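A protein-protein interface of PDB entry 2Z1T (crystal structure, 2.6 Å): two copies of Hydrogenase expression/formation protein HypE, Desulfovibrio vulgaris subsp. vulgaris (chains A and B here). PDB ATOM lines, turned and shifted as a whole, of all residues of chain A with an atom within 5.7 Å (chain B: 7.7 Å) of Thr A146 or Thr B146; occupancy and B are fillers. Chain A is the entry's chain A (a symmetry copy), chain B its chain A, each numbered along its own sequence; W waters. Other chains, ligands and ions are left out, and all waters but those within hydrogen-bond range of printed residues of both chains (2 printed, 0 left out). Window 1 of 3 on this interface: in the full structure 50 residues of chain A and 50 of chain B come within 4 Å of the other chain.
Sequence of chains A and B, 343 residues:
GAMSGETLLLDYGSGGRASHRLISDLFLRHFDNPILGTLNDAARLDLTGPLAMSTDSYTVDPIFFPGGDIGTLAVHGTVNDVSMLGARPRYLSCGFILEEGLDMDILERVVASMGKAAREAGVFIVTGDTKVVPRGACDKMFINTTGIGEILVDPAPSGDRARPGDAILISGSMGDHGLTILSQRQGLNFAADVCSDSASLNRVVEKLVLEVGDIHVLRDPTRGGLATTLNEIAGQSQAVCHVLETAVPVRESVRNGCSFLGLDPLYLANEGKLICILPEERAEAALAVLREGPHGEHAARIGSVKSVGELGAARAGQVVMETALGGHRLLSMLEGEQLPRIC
Water W1 lies within hydrogen-bond range of OG1 of Thr B55 (2.7 Å), OD1 of Asn A144 (2.8 Å), OG of Ser A93 (3.1 Å), OG1 of Thr A146 (3.3 Å) and OG1 of Thr B146 (3.4 Å). Water W2 lies within hydrogen-bond range of OG1 of Thr A55 (2.7 Å), OD1 of Asn B144 (2.8 Å), OG of Ser B93 (3.1 Å), OG1 of Thr B146 (3.3 Å) and OG1 of Thr A146 (3.4 Å).
Met A53 touches Ser B93, and with the chains exchanged Ser A93 touches Met B53. Thr A55 touches Ser B93, and with the chains exchanged Ser A93 touches Thr B55. Ser A93 touches Thr B146, and with the chains exchanged Thr A146 touches Ser B93. Thr B146 touches its own counterpart, Thr A146. 14 positions are printed for both chains. Of the 13 pairs that touch across the chains among the printed residues, 12 have their exchanged pair printed and touching as well.
The backbone carbonyl oxygen of Thr B145 is in hydrogen-bond range of the side-chain hydroxyl of Thr B55. The backbone NH (N) of Ser B93 is in hydrogen-bond range of the backbone carbonyl oxygen (O) of Thr B146 (2.8 Å). The side-chain hydroxyl of Thr A55 is in hydrogen-bond range of the side-chain amide nitrogen of Asn A144 (2.9 Å). OG1 of Thr A55 lies within hydrogen-bond range of O of Thr A145, at 3.4 Å. The side-chain hydroxyl (OG1) of Thr A55 sits at hydrogen-bond distance from the side-chain hydroxyl (OG1) of Thr A146 (2.9 Å). N of Ser A93 lies within hydrogen-bond range of O of Thr A146 (2.8 Å).
Printed residues of chain B within 4 Å of Ser A93: Met B53 (3.4 Å), Thr B55 (3.8 Å) and Thr B146 (3.7 Å). Printed residues of chain B within 4 Å of Cys A94: Thr B55 (3.7 Å). Thr A146 touches three residues of chain B. Of the printed residues of chain A, Cys B94 touches Thr A55 (3.7 Å). The nearest residue of chain B that does not touch Thr A146 is Asn B144 (4.3 Å). The nearest residue of chain A that does not touch Thr B146 is Asn A144 (4.3 Å). The nearest printed residue of chain A that does not touch Ser B93 is Ser A54 (5.4 Å).
Of the 26 printed residues of chain B, 7 touch a printed residue of chain A. Of the 14 printed residues of chain A, 6 touch a printed residue of chain B. Along chain A the printed residues that touch a printed residue of chain B span positions 53 to 146. Among the printed residues, 13 pairs touch across the chains.
Among the printed residues, pairs that only touch across the chains: Met A53 with Ser B93, Met A53 with Thr B127, Met A53 with Thr B146, Thr A55 with Ser B93, Thr A55 with Cys B94, Ser A93 with Met B53, Ser A93 with Thr B55, Ser A93 with Thr B146, Cys A94 with Thr B55, Thr A146 with Met B53 and Thr A146 with Ser B93.
The side-chain amide oxygen (OD1) of Asn A144 lies close to the side-chain amide oxygen (OD1) of Asn B144 (2.8 Å). OG1 of Thr B146 sits at hydrogen-bond distance from OG1 of Thr A146, 3.0 Å away.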
ATOM      1  N   MET A  53     -15.243  13.358  25.526  1.00  0.00           N
ATOM      2  CA  MET A  53     -14.723  14.610  26.041  1.00  0.00           C
ATOM      3  C   MET A  53     -14.970  15.758  25.093  1.00  0.00           C
ATOM      4  O   MET A  53     -14.751  15.656  23.868  1.00  0.00           O
ATOM      5  CB  MET A  53     -13.217  14.500  26.308  1.00  0.00           C
ATOM      6  CG  MET A  53     -12.540  15.836  26.690  1.00  0.00           C
ATOM      7  SD  MET A  53     -10.815  15.588  27.106  1.00  0.00           S
ATOM      8  CE  MET A  53     -10.473  16.992  28.126  1.00  0.00           C
ATOM      9  N   SER A  54     -15.356  16.890  25.644  1.00  0.00           N
ATOM     10  CA  SER A  54     -15.649  17.993  24.768  1.00  0.00           C
ATOM     11  C   SER A  54     -15.331  19.321  25.426  1.00  0.00           C
ATOM     12  O   SER A  54     -15.444  19.441  26.642  1.00  0.00           O
ATOM     13  CB  SER A  54     -17.118  17.915  24.392  1.00  0.00           C
ATOM     14  OG  SER A  54     -17.580  19.190  24.040  1.00  0.00           O
ATOM     15  N   THR A  55     -14.946  20.315  24.631  1.00  0.00           N
ATOM     16  CA  THR A  55     -14.640  21.640  25.153  1.00  0.00           C
ATOM     17  C   THR A  55     -15.268  22.747  24.324  1.00  0.00           C
ATOM     18  O   THR A  55     -15.381  22.632  23.100  1.00  0.00           O
ATOM     19  CB  THR A  55     -13.103  21.901  25.322  1.00  0.00           C
ATOM     20  OG1 THR A  55     -12.900  23.088  26.124  1.00  0.00           O
ATOM     21  CG2 THR A  55     -12.438  22.117  23.980  1.00  0.00           C
ATOM     22  N   ASP A  56     -15.660  23.827  25.001  1.00  0.00           N
ATOM     23  CA  ASP A  56     -16.251  24.970  24.335  1.00  0.00           C
ATOM     24  C   ASP A  56     -15.937  26.223  25.078  1.00  0.00           C
ATOM     25  O   ASP A  56     -15.910  26.236  26.337  1.00  0.00           O
ATOM     26  CB  ASP A  56     -17.755  24.861  24.329  1.00  0.00           C
ATOM     27  CG  ASP A  56     -18.287  24.460  23.022  1.00  0.00           C
ATOM     28  OD1 ASP A  56     -18.173  25.252  22.034  1.00  0.00           O
ATOM     29  OD2 ASP A  56     -18.834  23.341  22.988  1.00  0.00           O
ATOM     30  N   THR A  78     -22.087  22.440  26.675  1.00  0.00           N
ATOM     31  CA  THR A  78     -21.065  21.447  26.889  1.00  0.00           C
ATOM     32  C   THR A  78     -21.658  20.099  27.306  1.00  0.00           C
ATOM     33  O   THR A  78     -21.170  19.032  26.896  1.00  0.00           O
ATOM     34  CB  THR A  78     -20.009  21.973  27.849  1.00  0.00           C
ATOM     35  OG1 THR A  78     -19.317  23.072  27.206  1.00  0.00           O
ATOM     36  CG2 THR A  78     -19.026  20.885  28.173  1.00  0.00           C
ATOM     37  N   TYR A  91     -19.066  15.114  34.452  1.00  0.00           N
ATOM     38  CA  TYR A  91     -18.218  16.174  35.041  1.00  0.00           C
ATOM     39  C   TYR A  91     -17.830  17.284  34.089  1.00  0.00           C
ATOM     40  O   TYR A  91     -17.502  17.041  32.926  1.00  0.00           O
ATOM     41  CB  TYR A  91     -16.966  15.586  35.713  1.00  0.00           C
ATOM     42  CG  TYR A  91     -17.306  14.560  36.771  1.00  0.00           C
ATOM     43  CD1 TYR A  91     -17.901  14.946  37.971  1.00  0.00           C
ATOM     44  CD2 TYR A  91     -17.075  13.203  36.562  1.00  0.00           C
ATOM     45  CE1 TYR A  91     -18.246  14.019  38.951  1.00  0.00           C
ATOM     46  CE2 TYR A  91     -17.417  12.259  37.541  1.00  0.00           C
ATOM     47  CZ  TYR A  91     -18.007  12.684  38.729  1.00  0.00           C
ATOM     48  OH  TYR A  91     -18.366  11.785  39.689  1.00  0.00           O
ATOM     49  N   LEU A  92     -17.909  18.507  34.595  1.00  0.00           N
ATOM     50  CA  LEU A  92     -17.534  19.700  33.853  1.00  0.00           C
ATOM     51  C   LEU A  92     -16.400  20.321  34.594  1.00  0.00           C
ATOM     52  O   LEU A  92     -16.332  20.226  35.816  1.00  0.00           O
ATOM     53  CB  LEU A  92     -18.681  20.697  33.870  1.00  0.00           C
ATOM     54  CG  LEU A  92     -19.841  20.683  32.873  1.00  0.00           C
ATOM     55  CD1 LEU A  92     -19.511  21.685  31.852  1.00  0.00           C
ATOM     56  CD2 LEU A  92     -20.097  19.338  32.220  1.00  0.00           C
ATOM     57  N   SER A  93     -15.508  20.866  33.887  1.00  0.00           N
ATOM     58  CA  SER A  93     -14.514  21.774  34.445  1.00  0.00           C
ATOM     59  C   SER A  93     -14.746  23.228  33.932  1.00  0.00           C
ATOM     60  O   SER A  93     -15.450  23.306  32.899  1.00  0.00           O
ATOM     61  CB  SER A  93     -13.107  21.338  34.029  1.00  0.00           C
ATOM     62  OG  SER A  93     -12.932  21.447  32.627  1.00  0.00           O
ATOM     63  N   CYS A  94     -14.290  24.262  34.569  1.00  0.00           N
ATOM     64  CA  CYS A  94     -14.684  25.493  33.980  1.00  0.00           C
ATOM     65  C   CYS A  94     -13.685  26.632  34.199  1.00  0.00           C
ATOM     66  O   CYS A  94     -13.030  26.710  35.230  1.00  0.00           O
ATOM     67  CB  CYS A  94     -16.113  25.908  34.326  1.00  0.00           C
ATOM     68  SG  CYS A  94     -16.184  27.163  35.542  1.00  0.00           S
ATOM     69  N   ASN A 144     -14.734  29.095  29.310  1.00  0.00           N
ATOM     70  CA  ASN A 144     -14.575  27.818  28.659  1.00  0.00           C
ATOM     71  C   ASN A 144     -15.093  26.769  29.630  1.00  0.00           C
ATOM     72  O   ASN A 144     -14.918  26.902  30.836  1.00  0.00           O
ATOM     73  CB  ASN A 144     -13.115  27.542  28.292  1.00  0.00           C
ATOM     74  CG  ASN A 144     -12.905  26.127  27.810  1.00  0.00           C
ATOM     75  OD1 ASN A 144     -12.689  25.207  28.612  1.00  0.00           O
ATOM     76  ND2 ASN A 144     -12.999  25.923  26.482  1.00  0.00           N
ATOM     77  N   THR A 145     -15.738  25.731  29.122  1.00  0.00           N
ATOM     78  CA  THR A 145     -16.061  24.601  29.974  1.00  0.00           C
ATOM     79  C   THR A 145     -15.712  23.365  29.199  1.00  0.00           C
ATOM     80  O   THR A 145     -15.703  23.364  27.943  1.00  0.00           O
ATOM     81  CB  THR A 145     -17.546  24.533  30.376  1.00  0.00           C
ATOM     82  OG1 THR A 145     -18.361  24.484  29.200  1.00  0.00           O
ATOM     83  CG2 THR A 145     -17.956  25.737  31.235  1.00  0.00           C
ATOM     84  N   THR A 146     -15.403  22.307  29.943  1.00  0.00           N
ATOM     85  CA  THR A 146     -14.966  21.078  29.303  1.00  0.00           C
ATOM     86  C   THR A 146     -15.719  20.016  29.994  1.00  0.00           C
ATOM     87  O   THR A 146     -15.749  19.994  31.199  1.00  0.00           O
ATOM     88  CB  THR A 146     -13.455  20.877  29.477  1.00  0.00           C
ATOM     89  OG1 THR A 146     -12.788  21.944  28.794  1.00  0.00           O
ATOM     90  CG2 THR A 146     -13.004  19.512  28.920  1.00  0.00           C
ATOM     91  N   GLY A 147     -16.363  19.158  29.229  1.00  0.00           N
ATOM     92  CA  GLY A 147     -17.216  18.163  29.818  1.00  0.00           C
ATOM     93  C   GLY A 147     -16.602  16.810  29.675  1.00  0.00           C
ATOM     94  O   GLY A 147     -15.828  16.572  28.757  1.00  0.00           O
ATOM     95  N   ILE A 148     -16.964  15.911  30.573  1.00  0.00           N
ATOM     96  CA  ILE A 148     -16.491  14.540  30.488  1.00  0.00           C
ATOM     97  C   ILE A 148     -17.605  13.578  30.888  1.00  0.00           C
ATOM     98  O   ILE A 148     -18.345  13.814  31.864  1.00  0.00           O
ATOM     99  CB  ILE A 148     -15.212  14.359  31.339  1.00  0.00           C
ATOM    100  CG1 ILE A 148     -13.983  14.300  30.424  1.00  0.00           C
ATOM    101  CG2 ILE A 148     -15.287  13.107  32.157  1.00  0.00           C
ATOM    102  CD1 ILE A 148     -13.474  12.861  30.161  1.00  0.00           C
ATOM    103  N   ALA B  52      -7.376  12.021  36.852  1.00  0.00           N
ATOM    104  CA  ALA B  52      -7.169  13.381  37.323  1.00  0.00           C
ATOM    105  C   ALA B  52      -7.582  14.358  36.220  1.00  0.00           C
ATOM    106  O   ALA B  52      -7.300  14.122  35.038  1.00  0.00           O
ATOM    107  CB  ALA B  52      -5.719  13.580  37.695  1.00  0.00           C
ATOM    108  N   MET B  53      -8.263  15.439  36.586  1.00  0.00           N
ATOM    109  CA  MET B  53      -8.692  16.407  35.596  1.00  0.00           C
ATOM    110  C   MET B  53      -8.341  17.820  35.996  1.00  0.00           C
ATOM    111  O   MET B  53      -8.547  18.244  37.152  1.00  0.00           O
ATOM    112  CB  MET B  53     -10.207  16.315  35.372  1.00  0.00           C
ATOM    113  CG  MET B  53     -10.784  17.427  34.466  1.00  0.00           C
ATOM    114  SD  MET B  53     -12.530  17.166  34.159  1.00  0.00           S
ATOM    115  CE  MET B  53     -12.779  18.053  32.650  1.00  0.00           C
ATOM    116  N   SER B  54      -7.877  18.594  35.037  1.00  0.00           N
ATOM    117  CA  SER B  54      -7.485  19.932  35.392  1.00  0.00           C
ATOM    118  C   SER B  54      -7.710  20.896  34.244  1.00  0.00           C
ATOM    119  O   SER B  54      -7.608  20.500  33.086  1.00  0.00           O
ATOM    120  CB  SER B  54      -6.020  19.900  35.791  1.00  0.00           C
ATOM    121  OG  SER B  54      -5.455  21.169  35.599  1.00  0.00           O
ATOM    122  N   THR B  55      -8.003  22.155  34.556  1.00  0.00           N
ATOM    123  CA  THR B  55      -8.214  23.170  33.534  1.00  0.00           C
ATOM    124  C   THR B  55      -7.488  24.467  33.849  1.00  0.00           C
ATOM    125  O   THR B  55      -7.364  24.853  35.015  1.00  0.00           O
ATOM    126  CB  THR B  55      -9.728  23.459  33.248  1.00  0.00           C
ATOM    127  OG1 THR B  55      -9.852  24.227  32.028  1.00  0.00           O
ATOM    128  CG2 THR B  55     -10.353  24.254  34.373  1.00  0.00           C
ATOM    129  N   ASP B  56      -7.025  25.142  32.798  1.00  0.00           N
ATOM    130  CA  ASP B  56      -6.336  26.407  32.948  1.00  0.00           C
ATOM    131  C   ASP B  56      -6.563  27.269  31.753  1.00  0.00           C
ATOM    132  O   ASP B  56      -6.611  26.769  30.597  1.00  0.00           O
ATOM    133  CB  ASP B  56      -4.845  26.195  33.023  1.00  0.00           C
ATOM    134  CG  ASP B  56      -4.324  26.322  34.388  1.00  0.00           C
ATOM    135  OD1 ASP B  56      -4.360  27.455  34.965  1.00  0.00           O
ATOM    136  OD2 ASP B  56      -3.865  25.276  34.885  1.00  0.00           O
ATOM    137  N   SER B  57      -6.661  28.566  32.022  1.00  0.00           N
ATOM    138  CA  SER B  57      -6.672  29.526  30.948  1.00  0.00           C
ATOM    139  C   SER B  57      -5.378  30.300  30.967  1.00  0.00           C
ATOM    140  O   SER B  57      -4.757  30.442  31.996  1.00  0.00           O
ATOM    141  CB  SER B  57      -7.901  30.417  31.025  1.00  0.00           C
ATOM    142  OG  SER B  57      -9.073  29.618  30.846  1.00  0.00           O
ATOM    143  N   TYR B  58      -4.951  30.766  29.810  1.00  0.00           N
ATOM    144  CA  TYR B  58      -3.645  31.336  29.651  1.00  0.00           C
ATOM    145  C   TYR B  58      -3.818  32.699  29.014  1.00  0.00           C
ATOM    146  O   TYR B  58      -4.372  32.821  27.912  1.00  0.00           O
ATOM    147  CB  TYR B  58      -2.775  30.384  28.828  1.00  0.00           C
ATOM    148  CG  TYR B  58      -2.517  29.087  29.570  1.00  0.00           C
ATOM    149  CD1 TYR B  58      -3.374  28.014  29.424  1.00  0.00           C
ATOM    150  CD2 TYR B  58      -1.433  28.954  30.462  1.00  0.00           C
ATOM    151  CE1 TYR B  58      -3.172  26.830  30.112  1.00  0.00           C
ATOM    152  CE2 TYR B  58      -1.212  27.770  31.157  1.00  0.00           C
ATOM    153  CZ  TYR B  58      -2.091  26.713  30.975  1.00  0.00           C
ATOM    154  OH  TYR B  58      -1.932  25.517  31.645  1.00  0.00           O
ATOM    155  N   ALA B  74       0.482  26.823  27.776  1.00  0.00           N
ATOM    156  CA  ALA B  74      -0.807  26.172  27.581  1.00  0.00           C
ATOM    157  C   ALA B  74      -0.717  24.641  27.635  1.00  0.00           C
ATOM    158  O   ALA B  74      -1.551  23.990  28.283  1.00  0.00           O
ATOM    159  CB  ALA B  74      -1.422  26.644  26.286  1.00  0.00           C
ATOM    160  N   THR B  78      -0.754  22.699  31.942  1.00  0.00           N
ATOM    161  CA  THR B  78      -1.853  21.787  32.136  1.00  0.00           C
ATOM    162  C   THR B  78      -1.374  20.345  32.315  1.00  0.00           C
ATOM    163  O   THR B  78      -1.936  19.580  33.117  1.00  0.00           O
ATOM    164  CB  THR B  78      -2.881  21.956  31.027  1.00  0.00           C
ATOM    165  OG1 THR B  78      -3.475  23.271  31.153  1.00  0.00           O
ATOM    166  CG2 THR B  78      -3.950  20.910  31.160  1.00  0.00           C
ATOM    167  N   VAL B  79      -0.302  19.988  31.615  1.00  0.00           N
ATOM    168  CA  VAL B  79       0.344  18.704  31.852  1.00  0.00           C
ATOM    169  C   VAL B  79       0.756  18.610  33.330  1.00  0.00           C
ATOM    170  O   VAL B  79       0.512  17.611  34.024  1.00  0.00           O
ATOM    171  CB  VAL B  79       1.526  18.512  30.897  1.00  0.00           C
ATOM    172  CG1 VAL B  79       2.337  17.268  31.264  1.00  0.00           C
ATOM    173  CG2 VAL B  79       1.006  18.384  29.454  1.00  0.00           C
ATOM    174  N   VAL B  82      -2.178  18.250  35.954  1.00  0.00           N
ATOM    175  CA  VAL B  82      -2.752  16.912  35.987  1.00  0.00           C
ATOM    176  C   VAL B  82      -1.838  16.013  36.815  1.00  0.00           C
ATOM    177  O   VAL B  82      -2.313  15.327  37.727  1.00  0.00           O
ATOM    178  CB  VAL B  82      -2.988  16.388  34.574  1.00  0.00           C
ATOM    179  CG1 VAL B  82      -3.221  14.864  34.549  1.00  0.00           C
ATOM    180  CG2 VAL B  82      -4.149  17.115  33.929  1.00  0.00           C
ATOM    181  N   TYR B  91      -4.464  13.094  27.785  1.00  0.00           N
ATOM    182  CA  TYR B  91      -5.236  13.884  26.801  1.00  0.00           C
ATOM    183  C   TYR B  91      -5.521  15.312  27.210  1.00  0.00           C
ATOM    184  O   TYR B  91      -5.848  15.591  28.365  1.00  0.00           O
ATOM    185  CB  TYR B  91      -6.542  13.171  26.407  1.00  0.00           C
ATOM    186  CG  TYR B  91      -6.300  11.780  25.865  1.00  0.00           C
ATOM    187  CD1 TYR B  91      -5.697  11.595  24.622  1.00  0.00           C
ATOM    188  CD2 TYR B  91      -6.631  10.650  26.607  1.00  0.00           C
ATOM    189  CE1 TYR B  91      -5.441  10.325  24.113  1.00  0.00           C
ATOM    190  CE2 TYR B  91      -6.380   9.365  26.104  1.00  0.00           C
ATOM    191  CZ  TYR B  91      -5.780   9.221  24.857  1.00  0.00           C
ATOM    192  OH  TYR B  91      -5.507   7.983  24.353  1.00  0.00           O
ATOM    193  N   LEU B  92      -5.355  16.212  26.250  1.00  0.00           N
ATOM    194  CA  LEU B  92      -5.624  17.629  26.433  1.00  0.00           C
ATOM    195  C   LEU B  92      -6.719  17.980  25.486  1.00  0.00           C
ATOM    196  O   LEU B  92      -6.814  17.400  24.407  1.00  0.00           O
ATOM    197  CB  LEU B  92      -4.403  18.440  26.030  1.00  0.00           C
ATOM    198  CG  LEU B  92      -3.232  18.743  26.965  1.00  0.00           C
ATOM    199  CD1 LEU B  92      -3.466  20.098  27.483  1.00  0.00           C
ATOM    200  CD2 LEU B  92      -3.071  17.767  28.114  1.00  0.00           C
ATOM    201  N   SER B  93      -7.554  18.833  25.893  1.00  0.00           N
ATOM    202  CA  SER B  93      -8.483  19.509  24.997  1.00  0.00           C
ATOM    203  C   SER B  93      -8.131  21.023  24.874  1.00  0.00           C
ATOM    204  O   SER B  93      -7.406  21.460  25.798  1.00  0.00           O
ATOM    205  CB  SER B  93      -9.913  19.391  25.531  1.00  0.00           C
ATOM    206  OG  SER B  93     -10.056  20.076  26.763  1.00  0.00           O
ATOM    207  N   CYS B  94      -8.516  21.738  23.863  1.00  0.00           N
ATOM    208  CA  CYS B  94      -8.017  23.067  23.905  1.00  0.00           C
ATOM    209  C   CYS B  94      -8.928  24.092  23.224  1.00  0.00           C
ATOM    210  O   CYS B  94      -9.592  23.792  22.240  1.00  0.00           O
ATOM    211  CB  CYS B  94      -6.566  23.193  23.444  1.00  0.00           C
ATOM    212  SG  CYS B  94      -6.419  23.832  21.823  1.00  0.00           S
ATOM    213  N   GLY B  95      -8.959  25.304  23.765  1.00  0.00           N
ATOM    214  CA  GLY B  95      -9.958  26.278  23.344  1.00  0.00           C
ATOM    215  C   GLY B  95      -9.410  27.668  23.154  1.00  0.00           C
ATOM    216  O   GLY B  95      -9.158  28.339  24.114  1.00  0.00           O
ATOM    217  N   PHE B 124      -1.709  13.884  23.891  1.00  0.00           N
ATOM    218  CA  PHE B 124      -2.439  14.220  22.683  1.00  0.00           C
ATOM    219  C   PHE B 124      -3.516  15.258  22.915  1.00  0.00           C
ATOM    220  O   PHE B 124      -4.345  15.109  23.813  1.00  0.00           O
ATOM    221  CB  PHE B 124      -3.039  12.963  22.051  1.00  0.00           C
ATOM    222  CG  PHE B 124      -2.012  12.051  21.428  1.00  0.00           C
ATOM    223  CD1 PHE B 124      -1.760  12.099  20.056  1.00  0.00           C
ATOM    224  CD2 PHE B 124      -1.282  11.152  22.219  1.00  0.00           C
ATOM    225  CE1 PHE B 124      -0.794  11.264  19.465  1.00  0.00           C
ATOM    226  CE2 PHE B 124      -0.315  10.307  21.653  1.00  0.00           C
ATOM    227  CZ  PHE B 124      -0.078  10.361  20.259  1.00  0.00           C
ATOM    228  N   ILE B 125      -3.492  16.319  22.109  1.00  0.00           N
ATOM    229  CA  ILE B 125      -4.612  17.251  22.027  1.00  0.00           C
ATOM    230  C   ILE B 125      -5.700  16.600  21.181  1.00  0.00           C
ATOM    231  O   ILE B 125      -5.547  16.451  19.979  1.00  0.00           O
ATOM    232  CB  ILE B 125      -4.200  18.619  21.459  1.00  0.00           C
ATOM    233  CG1 ILE B 125      -3.227  19.296  22.426  1.00  0.00           C
ATOM    234  CG2 ILE B 125      -5.423  19.505  21.287  1.00  0.00           C
ATOM    235  CD1 ILE B 125      -2.243  20.234  21.780  1.00  0.00           C
ATOM    236  N   VAL B 126      -6.792  16.191  21.818  1.00  0.00           N
ATOM    237  CA  VAL B 126      -7.777  15.333  21.164  1.00  0.00           C
ATOM    238  C   VAL B 126      -9.027  16.042  20.673  1.00  0.00           C
ATOM    239  O   VAL B 126      -9.732  15.509  19.808  1.00  0.00           O
ATOM    240  CB  VAL B 126      -8.221  14.153  22.069  1.00  0.00           C
ATOM    241  CG1 VAL B 126      -7.056  13.245  22.375  1.00  0.00           C
ATOM    242  CG2 VAL B 126      -8.875  14.649  23.324  1.00  0.00           C
ATOM    243  N   THR B 127      -9.318  17.216  21.223  1.00  0.00           N
ATOM    244  CA  THR B 127     -10.505  17.967  20.846  1.00  0.00           C
ATOM    245  C   THR B 127     -10.255  19.449  21.097  1.00  0.00           C
ATOM    246  O   THR B 127      -9.341  19.809  21.855  1.00  0.00           O
ATOM    247  CB  THR B 127     -11.770  17.446  21.589  1.00  0.00           C
ATOM    248  OG1 THR B 127     -12.926  18.197  21.199  1.00  0.00           O
ATOM    249  CG2 THR B 127     -11.604  17.556  23.090  1.00  0.00           C
ATOM    250  N   ILE B 143      -6.059  31.188  25.654  1.00  0.00           N
ATOM    251  CA  ILE B 143      -6.184  29.749  25.445  1.00  0.00           C
ATOM    252  C   ILE B 143      -6.589  29.080  26.742  1.00  0.00           C
ATOM    253  O   ILE B 143      -5.996  29.330  27.780  1.00  0.00           O
ATOM    254  CB  ILE B 143      -4.840  29.130  24.970  1.00  0.00           C
ATOM    255  CG1 ILE B 143      -4.461  29.645  23.579  1.00  0.00           C
ATOM    256  CG2 ILE B 143      -4.904  27.599  24.956  1.00  0.00           C
ATOM    257  CD1 ILE B 143      -3.066  29.229  23.137  1.00  0.00           C
ATOM    258  N   ASN B 144      -7.610  28.247  26.698  1.00  0.00           N
ATOM    259  CA  ASN B 144      -7.857  27.363  27.811  1.00  0.00           C
ATOM    260  C   ASN B 144      -7.439  25.973  27.361  1.00  0.00           C
ATOM    261  O   ASN B 144      -7.623  25.615  26.203  1.00  0.00           O
ATOM    262  CB  ASN B 144      -9.328  27.375  28.234  1.00  0.00           C
ATOM    263  CG  ASN B 144      -9.640  26.302  29.249  1.00  0.00           C
ATOM    264  OD1 ASN B 144      -9.939  25.154  28.888  1.00  0.00           O
ATOM    265  ND2 ASN B 144      -9.539  26.651  30.545  1.00  0.00           N
ATOM    266  N   THR B 145      -6.868  25.186  28.259  1.00  0.00           N
ATOM    267  CA  THR B 145      -6.648  23.785  27.949  1.00  0.00           C
ATOM    268  C   THR B 145      -7.078  23.004  29.154  1.00  0.00           C
ATOM    269  O   THR B 145      -7.067  23.517  30.302  1.00  0.00           O
ATOM    270  CB  THR B 145      -5.179  23.444  27.634  1.00  0.00           C
ATOM    271  OG1 THR B 145      -4.351  23.816  28.741  1.00  0.00           O
ATOM    272  CG2 THR B 145      -4.691  24.156  26.365  1.00  0.00           C
ATOM    273  N   THR B 146      -7.481  21.762  28.903  1.00  0.00           N
ATOM    274  CA  THR B 146      -8.002  20.940  29.981  1.00  0.00           C
ATOM    275  C   THR B 146      -7.345  19.633  29.797  1.00  0.00           C
ATOM    276  O   THR B 146      -7.337  19.119  28.706  1.00  0.00           O
ATOM    277  CB  THR B 146      -9.526  20.803  29.879  1.00  0.00           C
ATOM    278  OG1 THR B 146     -10.097  22.104  30.056  1.00  0.00           O
ATOM    279  CG2 THR B 146     -10.073  19.825  30.938  1.00  0.00           C
ATOM    280  N   GLY B 147      -6.757  19.116  30.856  1.00  0.00           N
ATOM    281  CA  GLY B 147      -5.994  17.903  30.739  1.00  0.00           C
ATOM    282  C   GLY B 147      -6.709  16.779  31.411  1.00  0.00           C
ATOM    283  O   GLY B 147      -7.484  16.997  32.334  1.00  0.00           O
ATOM    284  N   ILE B 148      -6.432  15.566  30.965  1.00  0.00           N
ATOM    285  CA  ILE B 148      -7.009  14.391  31.594  1.00  0.00           C
ATOM    286  C   ILE B 148      -5.980  13.266  31.641  1.00  0.00           C
ATOM    287  O   ILE B 148      -5.241  13.024  30.666  1.00  0.00           O
ATOM    288  CB  ILE B 148      -8.312  13.978  30.871  1.00  0.00           C
ATOM    289  CG1 ILE B 148      -9.527  14.393  31.710  1.00  0.00           C
ATOM    290  CG2 ILE B 148      -8.349  12.500  30.637  1.00  0.00           C
ATOM    291  CD1 ILE B 148     -10.141  13.232  32.529  1.00  0.00           C
HETATM  292  O   HOH W   1     -12.471  24.218  31.203  1.00  0.00           O
HETATM  293  O   HOH W   2     -10.276  23.214  26.924  1.00  0.00           O
